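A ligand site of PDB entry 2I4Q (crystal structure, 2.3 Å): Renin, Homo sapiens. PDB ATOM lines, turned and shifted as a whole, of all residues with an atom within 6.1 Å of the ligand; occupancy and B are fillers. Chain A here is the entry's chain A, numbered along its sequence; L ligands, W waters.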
ATOM      1  N   THR A  14      18.257  19.758  13.495  1.00  0.00           N
ATOM      2  CA  THR A  14      18.643  20.907  12.683  1.00  0.00           C
ATOM      3  C   THR A  14      19.357  20.545  11.381  1.00  0.00           C
ATOM      4  O   THR A  14      19.404  21.367  10.462  1.00  0.00           O
ATOM      5  CB  THR A  14      19.554  21.861  13.483  1.00  0.00           C
ATOM      6  OG1 THR A  14      20.653  21.135  14.055  1.00  0.00           O
ATOM      7  CG2 THR A  14      18.822  22.467  14.689  1.00  0.00           C
ATOM      8  N   GLN A  15      19.925  19.343  11.311  1.00  0.00           N
ATOM      9  CA  GLN A  15      20.584  18.864  10.101  1.00  0.00           C
ATOM     10  C   GLN A  15      20.095  17.464   9.741  1.00  0.00           C
ATOM     11  O   GLN A  15      20.018  16.591  10.598  1.00  0.00           O
ATOM     12  CB  GLN A  15      22.104  18.871  10.276  1.00  0.00           C
ATOM     13  CG  GLN A  15      22.638  20.123  10.952  1.00  0.00           C
ATOM     14  CD  GLN A  15      24.138  20.157  11.020  1.00  0.00           C
ATOM     15  OE1 GLN A  15      24.818  19.461  10.272  1.00  0.00           O
ATOM     16  NE2 GLN A  15      24.676  20.974  11.926  1.00  0.00           N
ATOM     17  N   TYR A  16      19.758  17.274   8.467  1.00  0.00           N
ATOM     18  CA  TYR A  16      19.319  15.986   7.949  1.00  0.00           C
ATOM     19  C   TYR A  16      20.133  15.673   6.710  1.00  0.00           C
ATOM     20  O   TYR A  16      20.102  16.430   5.737  1.00  0.00           O
ATOM     21  CB  TYR A  16      17.825  16.013   7.604  1.00  0.00           C
ATOM     22  CG  TYR A  16      16.903  16.155   8.793  1.00  0.00           C
ATOM     23  CD1 TYR A  16      16.602  17.400   9.321  1.00  0.00           C
ATOM     24  CD2 TYR A  16      16.297  15.038   9.369  1.00  0.00           C
ATOM     25  CE1 TYR A  16      15.744  17.533  10.400  1.00  0.00           C
ATOM     26  CE2 TYR A  16      15.450  15.163  10.452  1.00  0.00           C
ATOM     27  CZ  TYR A  16      15.168  16.409  10.957  1.00  0.00           C
ATOM     28  OH  TYR A  16      14.318  16.551  12.029  1.00  0.00           O
ATOM     29  N   TYR A  17      20.859  14.560   6.737  1.00  0.00           N
ATOM     30  CA  TYR A  17      21.766  14.220   5.651  1.00  0.00           C
ATOM     31  C   TYR A  17      21.858  12.717   5.426  1.00  0.00           C
ATOM     32  O   TYR A  17      21.658  11.926   6.352  1.00  0.00           O
ATOM     33  CB  TYR A  17      23.162  14.789   5.941  1.00  0.00           C
ATOM     34  CG  TYR A  17      23.758  14.381   7.271  1.00  0.00           C
ATOM     35  CD1 TYR A  17      23.636  15.194   8.396  1.00  0.00           C
ATOM     36  CD2 TYR A  17      24.451  13.168   7.413  1.00  0.00           C
ATOM     37  CE1 TYR A  17      24.173  14.807   9.634  1.00  0.00           C
ATOM     38  CE2 TYR A  17      24.986  12.793   8.633  1.00  0.00           C
ATOM     39  CZ  TYR A  17      24.851  13.607   9.723  1.00  0.00           C
ATOM     40  OH  TYR A  17      25.396  13.223  10.924  1.00  0.00           O
ATOM     41  N   VAL A  32      23.312  17.017   2.512  1.00  0.00           N
ATOM     42  CA  VAL A  32      21.931  17.426   2.741  1.00  0.00           C
ATOM     43  C   VAL A  32      21.232  17.418   1.399  1.00  0.00           C
ATOM     44  O   VAL A  32      21.755  17.945   0.427  1.00  0.00           O
ATOM     45  CB  VAL A  32      21.878  18.855   3.309  1.00  0.00           C
ATOM     46  CG1 VAL A  32      20.434  19.333   3.430  1.00  0.00           C
ATOM     47  CG2 VAL A  32      22.594  18.919   4.664  1.00  0.00           C
ATOM     48  N   PHE A  33      20.043  16.834   1.337  1.00  0.00           N
ATOM     49  CA  PHE A  33      19.225  16.899   0.128  1.00  0.00           C
ATOM     50  C   PHE A  33      18.307  18.101   0.237  1.00  0.00           C
ATOM     51  O   PHE A  33      17.474  18.166   1.134  1.00  0.00           O
ATOM     52  CB  PHE A  33      18.446  15.604  -0.046  1.00  0.00           C
ATOM     53  CG  PHE A  33      19.317  14.406  -0.238  1.00  0.00           C
ATOM     54  CD1 PHE A  33      19.767  13.669   0.857  1.00  0.00           C
ATOM     55  CD2 PHE A  33      19.713  14.020  -1.511  1.00  0.00           C
ATOM     56  CE1 PHE A  33      20.580  12.560   0.672  1.00  0.00           C
ATOM     57  CE2 PHE A  33      20.537  12.904  -1.692  1.00  0.00           C
ATOM     58  CZ  PHE A  33      20.966  12.173  -0.600  1.00  0.00           C
ATOM     59  N   ASP A  34      18.454  19.020  -0.717  1.00  0.00           N
ATOM     60  CA  ASP A  34      18.075  20.425  -0.559  1.00  0.00           C
ATOM     61  C   ASP A  34      17.247  20.956  -1.726  1.00  0.00           C
ATOM     62  O   ASP A  34      17.783  21.290  -2.772  1.00  0.00           O
ATOM     63  CB  ASP A  34      19.378  21.236  -0.433  1.00  0.00           C
ATOM     64  CG  ASP A  34      19.147  22.736  -0.343  1.00  0.00           C
ATOM     65  OD1 ASP A  34      20.121  23.490  -0.562  1.00  0.00           O
ATOM     66  OD2 ASP A  34      18.044  23.240  -0.033  1.00  0.00           O
ATOM     67  N   THR A  35      15.930  21.091  -1.523  1.00  0.00           N
ATOM     68  CA  THR A  35      15.038  21.656  -2.537  1.00  0.00           C
ATOM     69  C   THR A  35      15.152  23.169  -2.702  1.00  0.00           C
ATOM     70  O   THR A  35      14.636  23.727  -3.669  1.00  0.00           O
ATOM     71  CB  THR A  35      13.573  21.293  -2.216  1.00  0.00           C
ATOM     72  OG1 THR A  35      13.241  21.689  -0.880  1.00  0.00           O
ATOM     73  CG2 THR A  35      13.367  19.779  -2.234  1.00  0.00           C
ATOM     74  N   GLY A  36      15.816  23.838  -1.756  1.00  0.00           N
ATOM     75  CA  GLY A  36      16.123  25.255  -1.868  1.00  0.00           C
ATOM     76  C   GLY A  36      17.343  25.645  -2.688  1.00  0.00           C
ATOM     77  O   GLY A  36      17.660  26.830  -2.803  1.00  0.00           O
ATOM     78  N   SER A  37      18.049  24.666  -3.248  1.00  0.00           N
ATOM     79  CA  SER A  37      19.166  24.910  -4.156  1.00  0.00           C
ATOM     80  C   SER A  37      19.205  23.823  -5.235  1.00  0.00           C
ATOM     81  O   SER A  37      18.486  22.842  -5.142  1.00  0.00           O
ATOM     82  CB  SER A  37      20.487  24.978  -3.389  1.00  0.00           C
ATOM     83  OG  SER A  37      20.829  23.697  -2.866  1.00  0.00           O
ATOM     84  N   TRP A  41      27.526  19.730  -4.464  1.00  0.00           N
ATOM     85  CA  TRP A  41      28.918  20.031  -4.134  1.00  0.00           C
ATOM     86  C   TRP A  41      29.401  19.212  -2.946  1.00  0.00           C
ATOM     87  O   TRP A  41      28.624  18.868  -2.065  1.00  0.00           O
ATOM     88  CB  TRP A  41      29.120  21.533  -3.877  1.00  0.00           C
ATOM     89  CG  TRP A  41      28.541  22.064  -2.594  1.00  0.00           C
ATOM     90  CD1 TRP A  41      27.322  22.647  -2.422  1.00  0.00           C
ATOM     91  CD2 TRP A  41      29.175  22.094  -1.300  1.00  0.00           C
ATOM     92  NE1 TRP A  41      27.151  23.025  -1.113  1.00  0.00           N
ATOM     93  CE2 TRP A  41      28.273  22.698  -0.403  1.00  0.00           C
ATOM     94  CE3 TRP A  41      30.414  21.652  -0.813  1.00  0.00           C
ATOM     95  CZ2 TRP A  41      28.564  22.879   0.947  1.00  0.00           C
ATOM     96  CZ3 TRP A  41      30.705  21.841   0.531  1.00  0.00           C
ATOM     97  CH2 TRP A  41      29.790  22.451   1.402  1.00  0.00           C
ATOM     98  N   TYR A  79      24.189  30.489  -0.310  1.00  0.00           N
ATOM     99  CA  TYR A  79      23.070  30.133   0.546  1.00  0.00           C
ATOM    100  C   TYR A  79      22.784  31.283   1.488  1.00  0.00           C
ATOM    101  O   TYR A  79      23.622  32.171   1.690  1.00  0.00           O
ATOM    102  CB  TYR A  79      23.357  28.862   1.341  1.00  0.00           C
ATOM    103  CG  TYR A  79      23.739  27.694   0.466  1.00  0.00           C
ATOM    104  CD1 TYR A  79      25.050  27.269   0.386  1.00  0.00           C
ATOM    105  CD2 TYR A  79      22.785  27.031  -0.283  1.00  0.00           C
ATOM    106  CE1 TYR A  79      25.407  26.210  -0.413  1.00  0.00           C
ATOM    107  CE2 TYR A  79      23.120  25.974  -1.095  1.00  0.00           C
ATOM    108  CZ  TYR A  79      24.442  25.565  -1.149  1.00  0.00           C
ATOM    109  OH  TYR A  79      24.789  24.506  -1.948  1.00  0.00           O
ATOM    110  N   SER A  80      21.608  31.262   2.093  1.00  0.00           N
ATOM    111  CA  SER A  80      21.155  32.330   2.969  1.00  0.00           C
ATOM    112  C   SER A  80      22.037  32.471   4.219  1.00  0.00           C
ATOM    113  O   SER A  80      22.156  33.551   4.769  1.00  0.00           O
ATOM    114  CB  SER A  80      19.689  32.125   3.360  1.00  0.00           C
ATOM    115  OG  SER A  80      19.512  30.897   4.031  1.00  0.00           O
ATOM    116  N   THR A  81      22.658  31.373   4.655  1.00  0.00           N
ATOM    117  CA  THR A  81      23.462  31.370   5.874  1.00  0.00           C
ATOM    118  C   THR A  81      24.968  31.213   5.612  1.00  0.00           C
ATOM    119  O   THR A  81      25.754  31.098   6.562  1.00  0.00           O
ATOM    120  CB  THR A  81      22.990  30.248   6.811  1.00  0.00           C
ATOM    121  OG1 THR A  81      23.010  28.988   6.121  1.00  0.00           O
ATOM    122  CG2 THR A  81      21.519  30.423   7.177  1.00  0.00           C
ATOM    123  N   GLY A  82      25.369  31.220   4.354  1.00  0.00           N
ATOM    124  CA  GLY A  82      26.767  30.995   4.017  1.00  0.00           C
ATOM    125  C   GLY A  82      27.042  30.694   2.558  1.00  0.00           C
ATOM    126  O   GLY A  82      26.132  30.417   1.781  1.00  0.00           O
ATOM    127  N   PRO A 114      29.649  29.164   8.522  1.00  0.00           N
ATOM    128  CA  PRO A 114      29.083  28.191   9.455  1.00  0.00           C
ATOM    129  C   PRO A 114      29.580  26.732   9.338  1.00  0.00           C
ATOM    130  O   PRO A 114      29.112  25.907  10.125  1.00  0.00           O
ATOM    131  CB  PRO A 114      27.616  28.207   9.046  1.00  0.00           C
ATOM    132  CG  PRO A 114      27.666  28.369   7.550  1.00  0.00           C
ATOM    133  CD  PRO A 114      28.889  29.200   7.249  1.00  0.00           C
ATOM    134  N   PHE A 115      30.456  26.399   8.411  1.00  0.00           N
ATOM    135  CA  PHE A 115      30.633  24.981   8.054  1.00  0.00           C
ATOM    136  C   PHE A 115      31.352  24.094   9.072  1.00  0.00           C
ATOM    137  O   PHE A 115      31.218  22.881   9.016  1.00  0.00           O
ATOM    138  CB  PHE A 115      31.198  24.837   6.639  1.00  0.00           C
ATOM    139  CG  PHE A 115      30.260  25.336   5.583  1.00  0.00           C
ATOM    140  CD1 PHE A 115      30.412  26.595   5.033  1.00  0.00           C
ATOM    141  CD2 PHE A 115      29.168  24.571   5.208  1.00  0.00           C
ATOM    142  CE1 PHE A 115      29.514  27.061   4.090  1.00  0.00           C
ATOM    143  CE2 PHE A 115      28.270  25.036   4.265  1.00  0.00           C
ATOM    144  CZ  PHE A 115      28.444  26.270   3.706  1.00  0.00           C
ATOM    145  N   LEU A 117      30.255  23.915  11.931  1.00  0.00           N
ATOM    146  CA  LEU A 117      29.088  23.440  12.673  1.00  0.00           C
ATOM    147  C   LEU A 117      28.289  22.386  11.896  1.00  0.00           C
ATOM    148  O   LEU A 117      27.325  21.834  12.402  1.00  0.00           O
ATOM    149  CB  LEU A 117      28.178  24.622  13.025  1.00  0.00           C
ATOM    150  CG  LEU A 117      28.798  25.659  13.953  1.00  0.00           C
ATOM    151  CD1 LEU A 117      28.041  26.970  13.893  1.00  0.00           C
ATOM    152  CD2 LEU A 117      28.848  25.125  15.386  1.00  0.00           C
ATOM    153  N   ALA A 118      28.715  22.131  10.662  1.00  0.00           N
ATOM    154  CA  ALA A 118      28.105  21.138   9.789  1.00  0.00           C
ATOM    155  C   ALA A 118      28.604  19.716  10.056  1.00  0.00           C
ATOM    156  O   ALA A 118      29.799  19.416   9.916  1.00  0.00           O
ATOM    157  CB  ALA A 118      28.371  21.498   8.327  1.00  0.00           C
ATOM    158  N   GLU A 119      27.683  18.838  10.451  1.00  0.00           N
ATOM    159  CA  GLU A 119      27.918  17.397  10.501  1.00  0.00           C
ATOM    160  C   GLU A 119      28.032  16.805   9.096  1.00  0.00           C
ATOM    161  O   GLU A 119      28.684  15.787   8.883  1.00  0.00           O
ATOM    162  CB  GLU A 119      26.803  16.708  11.285  1.00  0.00           C
ATOM    163  CG  GLU A 119      26.966  16.765  12.789  1.00  0.00           C
ATOM    164  CD  GLU A 119      27.685  15.548  13.339  1.00  0.00           C
ATOM    165  OE1 GLU A 119      28.660  15.107  12.705  1.00  0.00           O
ATOM    166  OE2 GLU A 119      27.259  15.019  14.405  1.00  0.00           O
ATOM    167  N   PHE A 120      27.370  17.436   8.146  1.00  0.00           N
ATOM    168  CA  PHE A 120      27.437  17.038   6.745  1.00  0.00           C
ATOM    169  C   PHE A 120      28.656  17.635   6.060  1.00  0.00           C
ATOM    170  O   PHE A 120      29.232  18.608   6.528  1.00  0.00           O
ATOM    171  CB  PHE A 120      26.155  17.448   6.012  1.00  0.00           C
ATOM    172  CG  PHE A 120      25.917  18.946   5.999  1.00  0.00           C
ATOM    173  CD1 PHE A 120      25.142  19.535   6.984  1.00  0.00           C
ATOM    174  CD2 PHE A 120      26.455  19.738   4.999  1.00  0.00           C
ATOM    175  CE1 PHE A 120      24.905  20.916   6.969  1.00  0.00           C
ATOM    176  CE2 PHE A 120      26.218  21.114   4.976  1.00  0.00           C
ATOM    177  CZ  PHE A 120      25.454  21.700   5.974  1.00  0.00           C
ATOM    178  N   GLY A 122      28.630  18.065   2.361  1.00  0.00           N
ATOM    179  CA  GLY A 122      28.188  18.780   1.186  1.00  0.00           C
ATOM    180  C   GLY A 122      26.676  18.807   1.025  1.00  0.00           C
ATOM    181  O   GLY A 122      25.944  18.566   1.973  1.00  0.00           O
ATOM    182  N   VAL A 123      26.225  19.147  -0.174  1.00  0.00           N
ATOM    183  CA  VAL A 123      24.803  19.333  -0.440  1.00  0.00           C
ATOM    184  C   VAL A 123      24.414  18.768  -1.808  1.00  0.00           C
ATOM    185  O   VAL A 123      25.182  18.834  -2.746  1.00  0.00           O
ATOM    186  CB  VAL A 123      24.430  20.828  -0.369  1.00  0.00           C
ATOM    187  CG1 VAL A 123      22.963  21.069  -0.770  1.00  0.00           C
ATOM    188  CG2 VAL A 123      24.711  21.384   1.028  1.00  0.00           C
ATOM    189  N   TYR A 158      11.243  13.671   7.551  1.00  0.00           N
ATOM    190  CA  TYR A 158      12.151  14.074   8.625  1.00  0.00           C
ATOM    191  C   TYR A 158      11.548  13.684   9.970  1.00  0.00           C
ATOM    192  O   TYR A 158      10.530  14.220  10.376  1.00  0.00           O
ATOM    193  CB  TYR A 158      12.384  15.588   8.597  1.00  0.00           C
ATOM    194  CG  TYR A 158      13.345  16.111   7.541  1.00  0.00           C
ATOM    195  CD1 TYR A 158      13.500  17.483   7.365  1.00  0.00           C
ATOM    196  CD2 TYR A 158      14.103  15.264   6.717  1.00  0.00           C
ATOM    197  CE1 TYR A 158      14.368  17.998   6.418  1.00  0.00           C
ATOM    198  CE2 TYR A 158      14.971  15.775   5.762  1.00  0.00           C
ATOM    199  CZ  TYR A 158      15.098  17.151   5.619  1.00  0.00           C
ATOM    200  OH  TYR A 158      15.956  17.684   4.685  1.00  0.00           O
ATOM    201  N   LEU A 220       8.398  28.997   0.011  1.00  0.00           N
ATOM    202  CA  LEU A 220       9.355  28.038  -0.529  1.00  0.00           C
ATOM    203  C   LEU A 220       9.405  26.821   0.388  1.00  0.00           C
ATOM    204  O   LEU A 220       9.610  26.962   1.588  1.00  0.00           O
ATOM    205  CB  LEU A 220      10.738  28.690  -0.635  1.00  0.00           C
ATOM    206  CG  LEU A 220      11.886  27.851  -1.190  1.00  0.00           C
ATOM    207  CD1 LEU A 220      11.796  27.760  -2.710  1.00  0.00           C
ATOM    208  CD2 LEU A 220      13.241  28.415  -0.759  1.00  0.00           C
ATOM    209  N   ASP A 222      11.471  24.107   1.609  1.00  0.00           N
ATOM    210  CA  ASP A 222      12.925  24.046   1.604  1.00  0.00           C
ATOM    211  C   ASP A 222      13.475  22.991   2.571  1.00  0.00           C
ATOM    212  O   ASP A 222      13.564  23.203   3.778  1.00  0.00           O
ATOM    213  CB  ASP A 222      13.446  25.437   1.980  1.00  0.00           C
ATOM    214  CG  ASP A 222      14.926  25.594   1.744  1.00  0.00           C
ATOM    215  OD1 ASP A 222      15.426  26.725   1.878  1.00  0.00           O
ATOM    216  OD2 ASP A 222      15.665  24.645   1.409  1.00  0.00           O
ATOM    217  N   THR A 223      13.886  21.854   2.025  1.00  0.00           N
ATOM    218  CA  THR A 223      14.362  20.728   2.826  1.00  0.00           C
ATOM    219  C   THR A 223      15.792  20.947   3.307  1.00  0.00           C
ATOM    220  O   THR A 223      16.286  20.189   4.136  1.00  0.00           O
ATOM    221  CB  THR A 223      14.290  19.414   2.041  1.00  0.00           C
ATOM    222  OG1 THR A 223      15.155  19.485   0.891  1.00  0.00           O
ATOM    223  CG2 THR A 223      12.884  19.187   1.461  1.00  0.00           C
ATOM    224  N   GLY A 224      16.448  21.981   2.778  1.00  0.00           N
ATOM    225  CA  GLY A 224      17.790  22.334   3.170  1.00  0.00           C
ATOM    226  C   GLY A 224      17.863  23.396   4.241  1.00  0.00           C
ATOM    227  O   GLY A 224      18.965  23.824   4.615  1.00  0.00           O
ATOM    228  N   ALA A 225      16.709  23.830   4.742  1.00  0.00           N
ATOM    229  CA  ALA A 225      16.638  24.815   5.812  1.00  0.00           C
ATOM    230  C   ALA A 225      16.211  24.109   7.096  1.00  0.00           C
ATOM    231  O   ALA A 225      15.297  23.301   7.068  1.00  0.00           O
ATOM    232  CB  ALA A 225      15.649  25.924   5.456  1.00  0.00           C
ATOM    233  N   SER A 226      16.889  24.407   8.200  1.00  0.00           N
ATOM    234  CA  SER A 226      16.543  23.827   9.502  1.00  0.00           C
ATOM    235  C   SER A 226      15.164  24.274   9.975  1.00  0.00           C
ATOM    236  O   SER A 226      14.395  23.472  10.486  1.00  0.00           O
ATOM    237  CB  SER A 226      17.539  24.257  10.582  1.00  0.00           C
ATOM    238  OG  SER A 226      18.860  23.885  10.251  1.00  0.00           O
ATOM    239  N   ALA A 313      12.732  22.247   7.943  1.00  0.00           N
ATOM    240  CA  ALA A 313      12.612  20.959   8.637  1.00  0.00           C
ATOM    241  C   ALA A 313      11.627  20.994   9.797  1.00  0.00           C
ATOM    242  O   ALA A 313      11.081  19.961  10.162  1.00  0.00           O
ATOM    243  CB  ALA A 313      13.974  20.491   9.114  1.00  0.00           C
HETATM  244  C1  LIG L   1      19.444  26.070   1.785  1.00  0.00           C
HETATM  245  C2  LIG L   1      22.133  22.650   2.936  1.00  0.00           C
HETATM  246  C3  LIG L   1      24.439  25.995   5.660  1.00  0.00           C
HETATM  247  C4  LIG L   1      22.940  24.737   6.850  1.00  0.00           C
HETATM  248  C5  LIG L   1      21.248  23.423   8.086  1.00  0.00           C
HETATM  249  C6  LIG L   1      19.788  21.652   7.144  1.00  0.00           C
HETATM  250  C7  LIG L   1      18.420  19.834   6.459  1.00  0.00           C
HETATM  251  C8  LIG L   1      24.419  25.697  11.320  1.00  0.00           C
HETATM  252  F1  LIG L   1      23.336  29.357   9.988  1.00  0.00           F
HETATM  253  C9  LIG L   1      23.692  28.154  10.383  1.00  0.00           C
HETATM  254  C10 LIG L   1      23.977  27.175   9.515  1.00  0.00           C
HETATM  255  C11 LIG L   1      23.791  27.854  11.807  1.00  0.00           C
HETATM  256  C12 LIG L   1      24.151  26.610  12.191  1.00  0.00           C
HETATM  257  F2  LIG L   1      24.215  26.385  13.491  1.00  0.00           F
HETATM  258  C13 LIG L   1      24.372  25.858  10.046  1.00  0.00           C
HETATM  259  C14 LIG L   1      24.687  24.705   9.093  1.00  0.00           C
HETATM  260  C15 LIG L   1      25.818  23.813   9.611  1.00  0.00           C
HETATM  261  C16 LIG L   1      23.395  23.921   9.010  1.00  0.00           C
HETATM  262  O1  LIG L   1      23.056  23.241   9.977  1.00  0.00           O
HETATM  263  N1  LIG L   1      22.594  23.996   7.934  1.00  0.00           N
HETATM  264  C17 LIG L   1      21.232  22.081   7.363  1.00  0.00           C
HETATM  265  O2  LIG L   1      19.695  20.238   6.973  1.00  0.00           O
HETATM  266  C18 LIG L   1      22.074  24.913   5.843  1.00  0.00           C
HETATM  267  C19 LIG L   1      24.147  25.311   6.710  1.00  0.00           C
HETATM  268  O3  LIG L   1      25.107  25.143   7.792  1.00  0.00           O
HETATM  269  C20 LIG L   1      23.698  26.183   4.726  1.00  0.00           C
HETATM  270  C21 LIG L   1      22.523  25.706   4.705  1.00  0.00           C
HETATM  271  C22 LIG L   1      21.476  25.835   3.635  1.00  0.00           C
HETATM  272  C23 LIG L   1      21.439  25.008   2.520  1.00  0.00           C
HETATM  273  C24 LIG L   1      22.504  23.959   2.262  1.00  0.00           C
HETATM  274  C25 LIG L   1      20.360  26.824   3.801  1.00  0.00           C
HETATM  275  N2  LIG L   1      20.292  27.664   4.863  1.00  0.00           N
HETATM  276  N3  LIG L   1      19.408  26.888   2.860  1.00  0.00           N
HETATM  277  N4  LIG L   1      20.441  25.155   1.612  1.00  0.00           N
HETATM  278  N5  LIG L   1      18.459  26.173   0.857  1.00  0.00           N
HETATM  279  O   HOH W   1      22.594  23.610  13.158  1.00  0.00           O
HETATM  280  O   HOH W   2      19.637  26.689   7.996  1.00  0.00           O
HETATM  281  O   HOH W   3      19.440  29.400   0.969  1.00  0.00           O
HETATM  282  O   HOH W   4      21.887  25.713  15.934  1.00  0.00           O
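N of Tyr 16 lies within hydrogen-bond range of O2 of the ligand, 3.3 Å away. The side-chain carboxylate of Asp 34 lies within hydrogen-bond range of a nitrogen (N4) of the ligand, 2.8 Å away. N2 of the ligand sits at hydrogen-bond distance from OG of Ser 80 (3.4 Å). OG1 of Thr 81 sits close to N2 of the ligand. The side-chain carboxylate (OD2) of Asp 222 lies within hydrogen-bond range of a nitrogen (N5) of the ligand, 3.2 Å away. NE2 of Gln 15 sits close to O1 of the ligand (3.4 Å).
Water W3 bridges N of Ser 80 (3.1 Å) and N3 of the ligand (3.1 Å). Water W1 bridges an oxygen (O1) of the ligand (3.2 Å) and the side-chain hydroxyl (OG1) of Thr 14 (3.3 Å).
NE2 of Gln 15 sits at hydrogen-bond distance from O of Leu 117 (2.8 Å). OD2 of Asp 34 lies close to N of Gly 224 (3.5 Å). N of Thr 223 is in hydrogen-bond range of OG1 of Thr 35, 3.0 Å away. The backbone carbonyl oxygen (O) of Val 123 sits at hydrogen-bond distance from the backbone NH (N) of Trp 41 (3.0 Å). N of Ala 313 lies within hydrogen-bond range of O of Ser 226 (3.3 Å). OH of Tyr 79 lies within hydrogen-bond range of NE1 of Trp 41 (2.9 Å). The side-chain carboxylate (OD1) of Asp 34 lies within hydrogen-bond range of the side-chain hydroxyl (OG) of Ser 37 (2.4 Å). The side-chain hydroxyl (OG1) of Thr 223 is in hydrogen-bond range of the backbone carbonyl oxygen (O) of Phe 33 (2.7 Å).
Residues that only touch the ligand: Thr 223 (3.2 Å), Ser 226 (3.3 Å), Thr 14 (3.4 Å), Gly 224 (3.4 Å), Val 123 (3.4 Å), Ala 118 (3.5 Å), Tyr 79 (3.6 Å), Leu 117 (3.7 Å), Val 32 (3.7 Å), Gly 36 (3.7 Å), Tyr 158 (3.7 Å), Pro 114 (3.8 Å) and Phe 120 (3.9 Å). Within 4 Å of the ligand: Thr 14, Gln 15, Tyr 16, Val 32, Asp 34, Gly 36, Tyr 79, Ser 80, Thr 81, Pro 114, Leu 117, Ala 118, Phe 120, Val 123, Tyr 158, Asp 222, Thr 223, Gly 224 and Ser 226. The nearest printed residue that does not touch the ligand is Phe 115 (4.2 Å).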
